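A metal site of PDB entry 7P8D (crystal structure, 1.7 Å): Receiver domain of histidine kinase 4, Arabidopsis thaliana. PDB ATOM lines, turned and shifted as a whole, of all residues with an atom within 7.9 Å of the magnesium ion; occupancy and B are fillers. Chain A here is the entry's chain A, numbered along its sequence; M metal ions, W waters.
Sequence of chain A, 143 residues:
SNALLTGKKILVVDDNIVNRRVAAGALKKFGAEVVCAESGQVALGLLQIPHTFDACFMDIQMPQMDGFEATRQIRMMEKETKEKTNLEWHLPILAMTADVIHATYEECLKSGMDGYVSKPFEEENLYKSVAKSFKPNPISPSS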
ATOM      1  N   VAL A  13       3.346 -22.917  16.997  1.00  0.00           N
ATOM      2  CA  VAL A  13       1.957 -22.556  16.716  1.00  0.00           C
ATOM      3  C   VAL A  13       1.667 -21.224  17.382  1.00  0.00           C
ATOM      4  O   VAL A  13       1.683 -21.133  18.618  1.00  0.00           O
ATOM      5  CB  VAL A  13       0.960 -23.616  17.222  1.00  0.00           C
ATOM      6  CG1 VAL A  13      -0.452 -23.286  16.736  1.00  0.00           C
ATOM      7  CG2 VAL A  13       1.430 -25.065  16.860  1.00  0.00           C
ATOM      8  N   ASP A  14       1.414 -20.183  16.583  1.00  0.00           N
ATOM      9  CA  ASP A  14       1.100 -18.850  17.098  1.00  0.00           C
ATOM     10  C   ASP A  14       0.385 -18.070  16.013  1.00  0.00           C
ATOM     11  O   ASP A  14       0.851 -18.036  14.864  1.00  0.00           O
ATOM     12  CB  ASP A  14       2.401 -18.130  17.500  1.00  0.00           C
ATOM     13  CG  ASP A  14       2.166 -16.996  18.479  1.00  0.00           C
ATOM     14  OD1 ASP A  14       1.436 -16.038  18.126  1.00  0.00           O
ATOM     15  OD2 ASP A  14       2.711 -17.071  19.608  1.00  0.00           O
ATOM     16  N   ASP A  15      -0.704 -17.382  16.367  1.00  0.00           N
ATOM     17  CA  ASP A  15      -1.399 -16.604  15.343  1.00  0.00           C
ATOM     18  C   ASP A  15      -0.693 -15.291  14.987  1.00  0.00           C
ATOM     19  O   ASP A  15      -1.068 -14.652  14.001  1.00  0.00           O
ATOM     20  CB  ASP A  15      -2.835 -16.333  15.757  1.00  0.00           C
ATOM     21  CG  ASP A  15      -2.937 -15.436  16.986  1.00  0.00           C
ATOM     22  OD1 ASP A  15      -2.328 -15.756  17.997  1.00  0.00           O
ATOM     23  OD2 ASP A  15      -3.617 -14.404  16.905  1.00  0.00           O
ATOM     24  N   ASN A  16       0.318 -14.885  15.743  1.00  0.00           N
ATOM     25  CA  ASN A  16       1.018 -13.619  15.481  1.00  0.00           C
ATOM     26  C   ASN A  16       2.301 -13.911  14.721  1.00  0.00           C
ATOM     27  O   ASN A  16       3.193 -14.573  15.253  1.00  0.00           O
ATOM     28  CB  ASN A  16       1.342 -12.898  16.797  1.00  0.00           C
ATOM     29  CG  ASN A  16       1.835 -11.476  16.587  1.00  0.00           C
ATOM     30  OD1 ASN A  16       2.641 -11.205  15.685  1.00  0.00           O
ATOM     31  ND2 ASN A  16       1.353 -10.565  17.399  1.00  0.00           N
ATOM     32  N   ASN A  19       5.688 -13.334  16.566  1.00  0.00           N
ATOM     33  CA  ASN A  19       6.074 -14.407  17.479  1.00  0.00           C
ATOM     34  C   ASN A  19       6.638 -15.596  16.722  1.00  0.00           C
ATOM     35  O   ASN A  19       7.638 -16.198  17.134  1.00  0.00           O
ATOM     36  CB  ASN A  19       4.891 -14.840  18.342  1.00  0.00           C
ATOM     37  CG  ASN A  19       4.632 -13.905  19.494  1.00  0.00           C
ATOM     38  OD1 ASN A  19       5.486 -13.114  19.882  1.00  0.00           O
ATOM     39  ND2 ASN A  19       3.442 -14.008  20.080  1.00  0.00           N
ATOM     40  N   GLU A  38      -0.062 -21.039  11.809  1.00  0.00           N
ATOM     41  CA  GLU A  38      -0.739 -19.805  12.209  1.00  0.00           C
ATOM     42  C   GLU A  38      -1.991 -20.052  13.060  1.00  0.00           C
ATOM     43  O   GLU A  38      -2.605 -19.085  13.535  1.00  0.00           O
ATOM     44  CB  GLU A  38      -1.075 -18.977  10.964  1.00  0.00           C
ATOM     45  CG  GLU A  38      -2.093 -19.574   9.959  1.00  0.00           C
ATOM     46  CD  GLU A  38      -1.454 -20.471   8.875  1.00  0.00           C
ATOM     47  OE1 GLU A  38      -0.448 -21.211   9.160  1.00  0.00           O
ATOM     48  OE2 GLU A  38      -1.976 -20.414   7.727  1.00  0.00           O
ATOM     49  N   ASP A  59       1.065 -21.416  21.392  1.00  0.00           N
ATOM     50  CA  ASP A  59       0.416 -20.188  21.844  1.00  0.00           C
ATOM     51  C   ASP A  59      -0.891 -20.518  22.562  1.00  0.00           C
ATOM     52  O   ASP A  59      -1.684 -21.336  22.100  1.00  0.00           O
ATOM     53  CB  ASP A  59       0.148 -19.323  20.601  1.00  0.00           C
ATOM     54  CG  ASP A  59      -0.466 -17.976  20.892  1.00  0.00           C
ATOM     55  OD1 ASP A  59      -0.412 -17.531  22.051  1.00  0.00           O
ATOM     56  OD2 ASP A  59      -0.981 -17.341  19.944  1.00  0.00           O
ATOM     57  N   ILE A  60      -1.162 -19.850  23.662  1.00  0.00           N
ATOM     58  CA  ILE A  60      -2.417 -20.239  24.315  1.00  0.00           C
ATOM     59  C   ILE A  60      -3.616 -19.453  23.766  1.00  0.00           C
ATOM     60  O   ILE A  60      -4.707 -20.021  23.661  1.00  0.00           O
ATOM     61  CB  ILE A  60      -2.306 -20.142  25.851  1.00  0.00           C
ATOM     62  CG1 ILE A  60      -1.926 -18.772  26.335  1.00  0.00           C
ATOM     63  CG2 ILE A  60      -1.276 -21.126  26.423  1.00  0.00           C
ATOM     64  CD1 ILE A  60      -1.984 -18.785  27.855  1.00  0.00           C
ATOM     65  N   GLN A  61      -3.454 -18.202  23.376  1.00  0.00           N
ATOM     66  CA  GLN A  61      -4.597 -17.371  22.983  1.00  0.00           C
ATOM     67  C   GLN A  61      -4.569 -17.219  21.483  1.00  0.00           C
ATOM     68  O   GLN A  61      -3.728 -16.493  20.931  1.00  0.00           O
ATOM     69  CB  GLN A  61      -4.582 -16.016  23.675  1.00  0.00           C
ATOM     70  CG  GLN A  61      -5.149 -16.087  25.097  1.00  0.00           C
ATOM     71  CD  GLN A  61      -5.702 -14.768  25.623  1.00  0.00           C
ATOM     72  OE1 GLN A  61      -5.112 -13.697  25.440  1.00  0.00           O
ATOM     73  NE2 GLN A  61      -6.854 -14.834  26.288  1.00  0.00           N
ATOM     74  N   MET A  62      -5.509 -17.899  20.824  1.00  0.00           N
ATOM     75  CA  MET A  62      -5.674 -17.804  19.382  1.00  0.00           C
ATOM     76  C   MET A  62      -7.159 -17.807  19.055  1.00  0.00           C
ATOM     77  O   MET A  62      -7.955 -18.458  19.746  1.00  0.00           O
ATOM     78  CB  MET A  62      -5.004 -18.991  18.651  1.00  0.00           C
ATOM     79  CG  MET A  62      -3.479 -19.154  18.919  1.00  0.00           C
ATOM     80  SD  MET A  62      -2.812 -20.520  17.989  1.00  0.00           S
ATOM     81  CE  MET A  62      -3.411 -21.953  18.898  1.00  0.00           C
ATOM     82  N   PRO A  63      -7.560 -17.098  18.004  1.00  0.00           N
ATOM     83  CA  PRO A  63      -8.973 -17.095  17.616  1.00  0.00           C
ATOM     84  C   PRO A  63      -9.379 -18.442  17.031  1.00  0.00           C
ATOM     85  O   PRO A  63      -8.546 -19.238  16.575  1.00  0.00           O
ATOM     86  CB  PRO A  63      -9.061 -15.972  16.592  1.00  0.00           C
ATOM     87  CG  PRO A  63      -7.689 -15.814  16.065  1.00  0.00           C
ATOM     88  CD  PRO A  63      -6.757 -16.176  17.178  1.00  0.00           C
ATOM     89  N   MET A  96       3.459 -21.267  25.161  1.00  0.00           N
ATOM     90  CA  MET A  96       4.040 -19.935  25.076  1.00  0.00           C
ATOM     91  C   MET A  96       3.102 -18.980  25.807  1.00  0.00           C
ATOM     92  O   MET A  96       2.006 -18.667  25.306  1.00  0.00           O
ATOM     93  CB  MET A  96       4.277 -19.521  23.620  1.00  0.00           C
ATOM     94  CG  MET A  96       5.348 -20.395  22.982  1.00  0.00           C
ATOM     95  SD  MET A  96       5.827 -19.882  21.333  1.00  0.00           S
ATOM     96  CE  MET A  96       4.348 -20.337  20.418  1.00  0.00           C
ATOM     97  N   ASP A  99       2.812 -13.885  25.985  1.00  0.00           N
ATOM     98  CA  ASP A  99       1.748 -12.992  25.516  1.00  0.00           C
ATOM     99  C   ASP A  99       0.731 -12.721  26.618  1.00  0.00           C
ATOM    100  O   ASP A  99       0.387 -11.571  26.891  1.00  0.00           O
ATOM    101  CB  ASP A  99       1.059 -13.588  24.287  1.00  0.00           C
ATOM    102  CG  ASP A  99       1.674 -13.139  22.952  1.00  0.00           C
ATOM    103  OD1 ASP A  99       2.906 -12.870  22.918  1.00  0.00           O
ATOM    104  OD2 ASP A  99       0.921 -13.060  21.949  1.00  0.00           O
ATOM    105  N   VAL A 100       0.200 -13.782  27.256  1.00  0.00           N
ATOM    106  CA  VAL A 100      -0.841 -13.560  28.269  1.00  0.00           C
ATOM    107  C   VAL A 100      -0.262 -12.859  29.491  1.00  0.00           C
ATOM    108  O   VAL A 100      -0.927 -12.024  30.128  1.00  0.00           O
ATOM    109  CB  VAL A 100      -1.537 -14.878  28.637  1.00  0.00           C
ATOM    110  CG1 VAL A 100      -2.467 -14.684  29.846  1.00  0.00           C
ATOM    111  CG2 VAL A 100      -2.319 -15.406  27.462  1.00  0.00           C
HETATM  112 MG    MG M   1      -1.991 -15.426  20.202  1.00  0.00          MG
HETATM  113  O   HOH W   1      -0.045 -14.418  19.728  1.00  0.00           O
HETATM  114  O   HOH W   2      -1.572 -14.421  22.211  1.00  0.00           O
HETATM  115  O   HOH W   3      -3.215 -13.678  19.860  1.00  0.00           O
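Water W3 is bound to the magnesium ion (2.2 Å).
The magnesium ion is bound by O of Gln 61, at 2.2 Å.
The magnesium ion is bound by OD2 of Asp 59 (2.2 Å).
Water W1 binds the magnesium ion (2.2 Å).
The magnesium ion is bound by OD1 of Asp 15.
The magnesium ion is bound by water W2 (2.3 Å).
Of the 14 residues printed, 3 come within 4 Å of the magnesium ion.
The backbone NH of Asp 59 sits at hydrogen-bond distance from the backbone carbonyl oxygen of Val 13, at 2.9 Å.
Water W2 bridges OD2 of Asp 99 (2.9 Å) and OD1 of Asp 59 (3.3 Å).
Water W1 bridges OD1 of Asp 14 and OD2 of Asp 99.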
